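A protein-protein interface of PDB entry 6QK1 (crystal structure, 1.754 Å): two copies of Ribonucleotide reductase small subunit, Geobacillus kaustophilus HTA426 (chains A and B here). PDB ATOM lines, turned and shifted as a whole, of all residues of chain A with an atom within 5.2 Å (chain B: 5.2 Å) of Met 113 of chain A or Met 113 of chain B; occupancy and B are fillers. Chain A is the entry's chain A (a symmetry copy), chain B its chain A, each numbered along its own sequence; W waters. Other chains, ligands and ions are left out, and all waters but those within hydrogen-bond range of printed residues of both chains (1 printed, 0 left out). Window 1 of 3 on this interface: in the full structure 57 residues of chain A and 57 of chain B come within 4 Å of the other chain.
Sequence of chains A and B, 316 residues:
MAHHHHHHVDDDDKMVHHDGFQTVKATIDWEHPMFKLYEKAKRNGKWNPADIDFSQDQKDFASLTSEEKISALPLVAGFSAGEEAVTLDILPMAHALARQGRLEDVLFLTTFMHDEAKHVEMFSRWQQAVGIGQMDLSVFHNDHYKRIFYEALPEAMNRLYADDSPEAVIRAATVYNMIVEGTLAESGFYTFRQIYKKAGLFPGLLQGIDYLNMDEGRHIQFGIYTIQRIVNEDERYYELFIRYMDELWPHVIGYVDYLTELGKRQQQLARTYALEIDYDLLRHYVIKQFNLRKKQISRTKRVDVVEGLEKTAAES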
ATOM      1  N   THR A  87     -23.514   2.111 -21.444  1.00  0.00           N
ATOM      2  CA  THR A  87     -22.652   2.438 -20.304  1.00  0.00           C
ATOM      3  C   THR A  87     -22.010   3.813 -20.484  1.00  0.00           C
ATOM      4  O   THR A  87     -21.968   4.626 -19.552  1.00  0.00           O
ATOM      5  CB  THR A  87     -21.568   1.355 -20.090  1.00  0.00           C
ATOM      6  OG1 THR A  87     -22.170   0.083 -19.854  1.00  0.00           O
ATOM      7  CG2 THR A  87     -20.763   1.672 -18.846  1.00  0.00           C
ATOM      8  N   ILE A  90     -25.095   6.968 -20.912  1.00  0.00           N
ATOM      9  CA  ILE A  90     -26.011   7.439 -19.892  1.00  0.00           C
ATOM     10  C   ILE A  90     -25.408   8.596 -19.116  1.00  0.00           C
ATOM     11  O   ILE A  90     -26.161   9.373 -18.506  1.00  0.00           O
ATOM     12  CB  ILE A  90     -26.406   6.282 -18.950  1.00  0.00           C
ATOM     13  CG1 ILE A  90     -27.574   6.655 -18.051  1.00  0.00           C
ATOM     14  CG2 ILE A  90     -25.224   5.788 -18.170  1.00  0.00           C
ATOM     15  CD1 ILE A  90     -28.854   6.955 -18.848  1.00  0.00           C
ATOM     16  N   LEU A  91     -24.077   8.756 -19.136  1.00  0.00           N
ATOM     17  CA  LEU A  91     -23.456   9.807 -18.319  1.00  0.00           C
ATOM     18  C   LEU A  91     -24.046  11.192 -18.555  1.00  0.00           C
ATOM     19  O   LEU A  91     -24.233  11.908 -17.569  1.00  0.00           O
ATOM     20  CB  LEU A  91     -21.932   9.850 -18.519  1.00  0.00           C
ATOM     21  CG  LEU A  91     -21.213   8.612 -17.980  1.00  0.00           C
ATOM     22  CD1 LEU A  91     -19.814   8.509 -18.582  1.00  0.00           C
ATOM     23  CD2 LEU A  91     -21.167   8.703 -16.469  1.00  0.00           C
ATOM     24  N   ALA A  94     -27.238  11.679 -16.476  1.00  0.00           N
ATOM     25  CA  ALA A  94     -26.944  11.869 -15.064  1.00  0.00           C
ATOM     26  C   ALA A  94     -26.511  13.301 -14.814  1.00  0.00           C
ATOM     27  O   ALA A  94     -26.963  13.940 -13.860  1.00  0.00           O
ATOM     28  CB  ALA A  94     -25.871  10.872 -14.618  1.00  0.00           C
ATOM     29  N   LEU A 109     -29.784   6.814 -10.876  1.00  0.00           N
ATOM     30  CA  LEU A 109     -28.943   6.613 -12.044  1.00  0.00           C
ATOM     31  C   LEU A 109     -27.600   5.976 -11.703  1.00  0.00           C
ATOM     32  O   LEU A 109     -27.020   5.325 -12.586  1.00  0.00           O
ATOM     33  CB  LEU A 109     -28.753   7.931 -12.800  1.00  0.00           C
ATOM     34  CG  LEU A 109     -30.023   8.270 -13.640  1.00  0.00           C
ATOM     35  CD1 LEU A 109     -29.920   9.659 -14.281  1.00  0.00           C
ATOM     36  CD2 LEU A 109     -30.353   7.230 -14.711  1.00  0.00           C
ATOM     37  N   THR A 110     -27.079   6.146 -10.489  1.00  0.00           N
ATOM     38  CA  THR A 110     -25.845   5.421 -10.132  1.00  0.00           C
ATOM     39  C   THR A 110     -26.059   3.913 -10.226  1.00  0.00           C
ATOM     40  O   THR A 110     -25.150   3.185 -10.673  1.00  0.00           O
ATOM     41  CB  THR A 110     -25.309   5.796  -8.726  1.00  0.00           C
ATOM     42  OG1 THR A 110     -26.158   5.266  -7.677  1.00  0.00           O
ATOM     43  CG2 THR A 110     -25.114   7.297  -8.557  1.00  0.00           C
ATOM     44  N   THR A 111     -27.275   3.430  -9.899  1.00  0.00           N
ATOM     45  CA  THR A 111     -27.564   1.993 -10.017  1.00  0.00           C
ATOM     46  C   THR A 111     -27.749   1.593 -11.469  1.00  0.00           C
ATOM     47  O   THR A 111     -27.305   0.503 -11.881  1.00  0.00           O
ATOM     48  CB  THR A 111     -28.797   1.579  -9.173  1.00  0.00           C
ATOM     49  OG1 THR A 111     -30.050   2.006  -9.761  1.00  0.00           O
ATOM     50  CG2 THR A 111     -28.691   2.122  -7.781  1.00  0.00           C
ATOM     51  N   PHE A 112     -28.332   2.494 -12.269  1.00  0.00           N
ATOM     52  CA  PHE A 112     -28.528   2.280 -13.691  1.00  0.00           C
ATOM     53  C   PHE A 112     -27.178   2.077 -14.372  1.00  0.00           C
ATOM     54  O   PHE A 112     -26.971   1.102 -15.133  1.00  0.00           O
ATOM     55  CB  PHE A 112     -29.283   3.507 -14.245  1.00  0.00           C
ATOM     56  CG  PHE A 112     -29.820   3.404 -15.645  1.00  0.00           C
ATOM     57  CD1 PHE A 112     -31.113   3.799 -15.900  1.00  0.00           C
ATOM     58  CD2 PHE A 112     -29.036   3.063 -16.722  1.00  0.00           C
ATOM     59  CE1 PHE A 112     -31.641   3.782 -17.168  1.00  0.00           C
ATOM     60  CE2 PHE A 112     -29.548   3.047 -18.006  1.00  0.00           C
ATOM     61  CZ  PHE A 112     -30.851   3.415 -18.247  1.00  0.00           C
ATOM     62  N   MET A 113     -26.237   2.987 -14.083  1.00  0.00           N
ATOM     63  CA  MET A 113     -24.914   2.953 -14.704  1.00  0.00           C
ATOM     64  C   MET A 113     -24.146   1.709 -14.277  1.00  0.00           C
ATOM     65  O   MET A 113     -23.498   1.055 -15.104  1.00  0.00           O
ATOM     66  CB  MET A 113     -24.151   4.218 -14.326  1.00  0.00           C
ATOM     67  CG  MET A 113     -24.786   5.414 -14.932  1.00  0.00           C
ATOM     68  SD  MET A 113     -23.882   6.989 -14.817  1.00  0.00           S
ATOM     69  CE  MET A 113     -24.107   7.344 -13.122  1.00  0.00           C
ATOM     70  N   HIS A 114     -24.188   1.388 -12.992  1.00  0.00           N
ATOM     71  CA  HIS A 114     -23.509   0.189 -12.504  1.00  0.00           C
ATOM     72  C   HIS A 114     -24.124  -1.088 -13.080  1.00  0.00           C
ATOM     73  O   HIS A 114     -23.397  -2.026 -13.437  1.00  0.00           O
ATOM     74  CB  HIS A 114     -23.472   0.128 -10.978  1.00  0.00           C
ATOM     75  CG  HIS A 114     -22.750  -1.097 -10.499  1.00  0.00           C
ATOM     76  ND1 HIS A 114     -21.429  -1.350 -10.829  1.00  0.00           N
ATOM     77  CD2 HIS A 114     -23.187  -2.191  -9.826  1.00  0.00           C
ATOM     78  CE1 HIS A 114     -21.073  -2.527 -10.331  1.00  0.00           C
ATOM     79  NE2 HIS A 114     -22.117  -3.061  -9.718  1.00  0.00           N
ATOM     80  N   ASP A 115     -25.449  -1.135 -13.244  1.00  0.00           N
ATOM     81  CA  ASP A 115     -26.070  -2.256 -13.958  1.00  0.00           C
ATOM     82  C   ASP A 115     -25.442  -2.433 -15.348  1.00  0.00           C
ATOM     83  O   ASP A 115     -25.038  -3.548 -15.733  1.00  0.00           O
ATOM     84  CB  ASP A 115     -27.589  -2.058 -14.122  1.00  0.00           C
ATOM     85  CG  ASP A 115     -28.396  -2.172 -12.799  1.00  0.00           C
ATOM     86  OD1 ASP A 115     -27.908  -2.618 -11.764  1.00  0.00           O
ATOM     87  OD2 ASP A 115     -29.565  -1.738 -12.815  1.00  0.00           O
ATOM     88  N   GLU A 116     -25.345  -1.334 -16.128  1.00  0.00           N
ATOM     89  CA  GLU A 116     -24.861  -1.462 -17.503  1.00  0.00           C
ATOM     90  C   GLU A 116     -23.427  -1.959 -17.521  1.00  0.00           C
ATOM     91  O   GLU A 116     -23.051  -2.736 -18.402  1.00  0.00           O
ATOM     92  CB  GLU A 116     -24.979  -0.132 -18.261  1.00  0.00           C
ATOM     93  CG  GLU A 116     -26.413   0.461 -18.338  1.00  0.00           C
ATOM     94  CD  GLU A 116     -27.413  -0.444 -19.079  1.00  0.00           C
ATOM     95  OE1 GLU A 116     -28.547  -0.029 -19.268  1.00  0.00           O
ATOM     96  OE2 GLU A 116     -27.062  -1.545 -19.550  1.00  0.00           O
ATOM     97  N   ALA A 117     -22.613  -1.499 -16.573  1.00  0.00           N
ATOM     98  CA  ALA A 117     -21.239  -1.981 -16.442  1.00  0.00           C
ATOM     99  C   ALA A 117     -21.205  -3.495 -16.255  1.00  0.00           C
ATOM    100  O   ALA A 117     -20.436  -4.203 -16.925  1.00  0.00           O
ATOM    101  CB  ALA A 117     -20.554  -1.307 -15.261  1.00  0.00           C
ATOM    102  N   THR B  87     -20.904  13.103  -5.095  1.00  0.00           N
ATOM    103  CA  THR B  87     -21.842  12.366  -5.947  1.00  0.00           C
ATOM    104  C   THR B  87     -22.089  13.114  -7.257  1.00  0.00           C
ATOM    105  O   THR B  87     -22.091  12.519  -8.341  1.00  0.00           O
ATOM    106  CB  THR B  87     -23.177  12.098  -5.212  1.00  0.00           C
ATOM    107  OG1 THR B  87     -22.952  11.341  -4.023  1.00  0.00           O
ATOM    108  CG2 THR B  87     -24.081  11.249  -6.082  1.00  0.00           C
ATOM    109  N   ILE B  90     -18.303  13.733  -9.478  1.00  0.00           N
ATOM    110  CA  ILE B  90     -17.488  12.718 -10.116  1.00  0.00           C
ATOM    111  C   ILE B  90     -17.915  12.509 -11.558  1.00  0.00           C
ATOM    112  O   ILE B  90     -17.110  12.006 -12.360  1.00  0.00           O
ATOM    113  CB  ILE B  90     -17.553  11.398  -9.319  1.00  0.00           C
ATOM    114  CG1 ILE B  90     -16.501  10.402  -9.781  1.00  0.00           C
ATOM    115  CG2 ILE B  90     -18.935  10.816  -9.344  1.00  0.00           C
ATOM    116  CD1 ILE B  90     -15.070  10.916  -9.556  1.00  0.00           C
ATOM    117  N   LEU B  91     -19.143  12.901 -11.926  1.00  0.00           N
ATOM    118  CA  LEU B  91     -19.620  12.626 -13.288  1.00  0.00           C
ATOM    119  C   LEU B  91     -18.679  13.128 -14.376  1.00  0.00           C
ATOM    120  O   LEU B  91     -18.495  12.399 -15.352  1.00  0.00           O
ATOM    121  CB  LEU B  91     -21.031  13.195 -13.516  1.00  0.00           C
ATOM    122  CG  LEU B  91     -22.111  12.491 -12.692  1.00  0.00           C
ATOM    123  CD1 LEU B  91     -23.368  13.353 -12.623  1.00  0.00           C
ATOM    124  CD2 LEU B  91     -22.390  11.141 -13.320  1.00  0.00           C
ATOM    125  N   ALA B  94     -15.868  10.591 -15.016  1.00  0.00           N
ATOM    126  CA  ALA B  94     -16.344   9.423 -15.741  1.00  0.00           C
ATOM    127  C   ALA B  94     -16.452   9.742 -17.220  1.00  0.00           C
ATOM    128  O   ALA B  94     -16.027   8.953 -18.069  1.00  0.00           O
ATOM    129  CB  ALA B  94     -17.687   8.966 -15.166  1.00  0.00           C
ATOM    130  N   LEU B 109     -15.579   3.318 -12.095  1.00  0.00           N
ATOM    131  CA  LEU B 109     -16.230   4.534 -11.640  1.00  0.00           C
ATOM    132  C   LEU B 109     -17.726   4.350 -11.404  1.00  0.00           C
ATOM    133  O   LEU B 109     -18.287   5.102 -10.592  1.00  0.00           O
ATOM    134  CB  LEU B 109     -15.962   5.684 -12.616  1.00  0.00           C
ATOM    135  CG  LEU B 109     -14.524   6.252 -12.412  1.00  0.00           C
ATOM    136  CD1 LEU B 109     -14.174   7.296 -13.479  1.00  0.00           C
ATOM    137  CD2 LEU B 109     -14.278   6.834 -11.019  1.00  0.00           C
ATOM    138  N   THR B 110     -18.390   3.415 -12.080  1.00  0.00           N
ATOM    139  CA  THR B 110     -19.806   3.162 -11.751  1.00  0.00           C
ATOM    140  C   THR B 110     -19.952   2.730 -10.295  1.00  0.00           C
ATOM    141  O   THR B 110     -20.920   3.136  -9.623  1.00  0.00           O
ATOM    142  CB  THR B 110     -20.466   2.116 -12.686  1.00  0.00           C
ATOM    143  OG1 THR B 110     -19.964   0.781 -12.426  1.00  0.00           O
ATOM    144  CG2 THR B 110     -20.315   2.473 -14.159  1.00  0.00           C
ATOM    145  N   THR B 111     -18.964   1.984  -9.759  1.00  0.00           N
ATOM    146  CA  THR B 111     -19.018   1.577  -8.347  1.00  0.00           C
ATOM    147  C   THR B 111     -18.691   2.743  -7.432  1.00  0.00           C
ATOM    148  O   THR B 111     -19.309   2.893  -6.360  1.00  0.00           O
ATOM    149  CB  THR B 111     -18.086   0.373  -8.055  1.00  0.00           C
ATOM    150  OG1 THR B 111     -16.685   0.741  -8.025  1.00  0.00           O
ATOM    151  CG2 THR B 111     -18.292  -0.712  -9.066  1.00  0.00           C
ATOM    152  N   PHE B 112     -17.778   3.615  -7.878  1.00  0.00           N
ATOM    153  CA  PHE B 112     -17.399   4.809  -7.143  1.00  0.00           C
ATOM    154  C   PHE B 112     -18.622   5.700  -6.946  1.00  0.00           C
ATOM    155  O   PHE B 112     -18.927   6.148  -5.815  1.00  0.00           O
ATOM    156  CB  PHE B 112     -16.286   5.514  -7.945  1.00  0.00           C
ATOM    157  CG  PHE B 112     -15.559   6.638  -7.262  1.00  0.00           C
ATOM    158  CD1 PHE B 112     -14.185   6.680  -7.314  1.00  0.00           C
ATOM    159  CD2 PHE B 112     -16.207   7.714  -6.701  1.00  0.00           C
ATOM    160  CE1 PHE B 112     -13.468   7.712  -6.759  1.00  0.00           C
ATOM    161  CE2 PHE B 112     -15.502   8.764  -6.143  1.00  0.00           C
ATOM    162  CZ  PHE B 112     -14.127   8.782  -6.174  1.00  0.00           C
ATOM    163  N   MET B 113     -19.348   5.945  -8.045  1.00  0.00           N
ATOM    164  CA  MET B 113     -20.514   6.827  -8.020  1.00  0.00           C
ATOM    165  C   MET B 113     -21.623   6.237  -7.159  1.00  0.00           C
ATOM    166  O   MET B 113     -22.260   6.953  -6.375  1.00  0.00           O
ATOM    167  CB  MET B 113     -20.999   7.057  -9.447  1.00  0.00           C
ATOM    168  CG  MET B 113     -19.998   7.829 -10.223  1.00  0.00           C
ATOM    169  SD  MET B 113     -20.497   8.431 -11.867  1.00  0.00           S
ATOM    170  CE  MET B 113     -20.486   6.929 -12.756  1.00  0.00           C
ATOM    171  N   HIS B 114     -21.880   4.946  -7.312  1.00  0.00           N
ATOM    172  CA  HIS B 114     -22.904   4.292  -6.499  1.00  0.00           C
ATOM    173  C   HIS B 114     -22.528   4.276  -5.016  1.00  0.00           C
ATOM    174  O   HIS B 114     -23.390   4.491  -4.152  1.00  0.00           O
ATOM    175  CB  HIS B 114     -23.214   2.879  -6.991  1.00  0.00           C
ATOM    176  CG  HIS B 114     -24.283   2.235  -6.158  1.00  0.00           C
ATOM    177  ND1 HIS B 114     -25.550   2.782  -6.034  1.00  0.00           N
ATOM    178  CD2 HIS B 114     -24.248   1.172  -5.316  1.00  0.00           C
ATOM    179  CE1 HIS B 114     -26.262   2.047  -5.189  1.00  0.00           C
ATOM    180  NE2 HIS B 114     -25.499   1.064  -4.738  1.00  0.00           N
ATOM    181  N   ASP B 115     -21.247   4.091  -4.688  1.00  0.00           N
ATOM    182  CA  ASP B 115     -20.805   4.249  -3.298  1.00  0.00           C
ATOM    183  C   ASP B 115     -21.211   5.625  -2.750  1.00  0.00           C
ATOM    184  O   ASP B 115     -21.802   5.732  -1.658  1.00  0.00           O
ATOM    185  CB  ASP B 115     -19.278   4.091  -3.163  1.00  0.00           C
ATOM    186  CG  ASP B 115     -18.762   2.643  -3.390  1.00  0.00           C
ATOM    187  OD1 ASP B 115     -19.513   1.672  -3.430  1.00  0.00           O
ATOM    188  OD2 ASP B 115     -17.537   2.508  -3.583  1.00  0.00           O
ATOM    189  N   GLU B 116     -20.902   6.705  -3.501  1.00  0.00           N
ATOM    190  CA  GLU B 116     -21.160   8.047  -2.978  1.00  0.00           C
ATOM    191  C   GLU B 116     -22.648   8.259  -2.760  1.00  0.00           C
ATOM    192  O   GLU B 116     -23.045   8.920  -1.797  1.00  0.00           O
ATOM    193  CB  GLU B 116     -20.594   9.127  -3.911  1.00  0.00           C
ATOM    194  CG  GLU B 116     -19.068   9.032  -4.185  1.00  0.00           C
ATOM    195  CD  GLU B 116     -18.207   9.190  -2.918  1.00  0.00           C
ATOM    196  OE1 GLU B 116     -16.990   9.216  -3.040  1.00  0.00           O
ATOM    197  OE2 GLU B 116     -18.729   9.368  -1.800  1.00  0.00           O
ATOM    198  N   ALA B 117     -23.475   7.728  -3.658  1.00  0.00           N
ATOM    199  CA  ALA B 117     -24.926   7.793  -3.496  1.00  0.00           C
ATOM    200  C   ALA B 117     -25.359   7.161  -2.176  1.00  0.00           C
ATOM    201  O   ALA B 117     -26.151   7.744  -1.419  1.00  0.00           O
ATOM    202  CB  ALA B 117     -25.618   7.083  -4.651  1.00  0.00           C
HETATM  203  O   HOH W   1     -22.790   4.482 -11.075  1.00  0.00           O
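The side-chain hydroxyl (OG1) of Thr 110 of chain B lies within hydrogen-bond range of a ring nitrogen (ND1) of His 114 of chain A (3.0 Å). ND1 of His 114 of chain B lies within hydrogen-bond range of OG1 of Thr 110 of chain A (3.0 Å).
Among the printed residues, merely in contact across the chains: Thr 111 of chain A with His 114 of chain B, His 114 of chain A with Thr 111 of chain B, Ala 117 of chain A with Thr 110 of chain B, Thr 110 of chain A with Ala 117 of chain B, Thr 110 of chain A with Met 113 of chain B, Met 113 of chain A with Thr 110 of chain B, Met 113 of chain A with Met 113 of chain B, Ala 94 of chain A with Leu 91 of chain B and Leu 91 of chain A with Ala 94 of chain B.
Of the printed residues of chain B, Met 113 of chain A touches Thr 110 (3.6 Å) and Met 113 (3.7 Å). Printed residues of chain A within 4 Å of Met 113 of chain B: Thr 110 and Met 113. Of the printed residues of chain B, Thr 110 of chain A touches Met 113 (3.6 Å), His 114 (3.0 Å) and Ala 117 (3.6 Å). Printed residues of chain B within 4 Å of His 114 of chain A: Thr 110 (3.0 Å) and Thr 111 (3.6 Å). Printed residues of chain A within 4 Å of Leu 91 of chain B: Ala 94. Printed residues of chain B within 4 Å of Thr 111 of chain A: His 114. Printed residues of chain B within 4 Å of Leu 91 of chain A: Ala 94. Phe 112 of chain B touches none of the printed residues of chain A. Thr 87 of chain B touches none of the printed residues of chain A. The nearest printed residue of chain A that does not touch Met 113 of chain B is Leu 91 of chain A (4.2 Å). The nearest printed residue of chain A that does not touch Thr 111 of chain B is Thr 110 of chain A (6.4 Å).
Hydrophobic or aromatic side chains of chain B that line the printed part of chain A: Leu 91, Ala 94, Met 113, His 114 and Ala 117. Of the 13 printed residues of chain A, 7 touch a printed residue of chain B. Among the printed residues, 11 pairs touch across the chains. Among the printed residues, no Asp or Glu carboxylate lies within 4 Å of a Lys or Arg side-chain nitrogen of the other chain.
Leu 91 of chain A touches Ala 94 of chain B, and with the chains exchanged Ala 94 of chain A touches Leu 91 of chain B. Thr 110 of chain A touches Met 113 of chain B, and with the chains exchanged Met 113 of chain A touches Thr 110 of chain B. Thr 110 of chain A touches Ala 117 of chain B, and with the chains exchanged Ala 117 of chain A touches Thr 110 of chain B. Thr 111 of chain A touches His 114 of chain B, and with the chains exchanged His 114 of chain A touches Thr 111 of chain B. 13 positions are printed for both chains.
Water W1 bridges O of Thr 110 of chain B (2.7 Å) and O of Thr 110 of chain A (2.7 Å).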
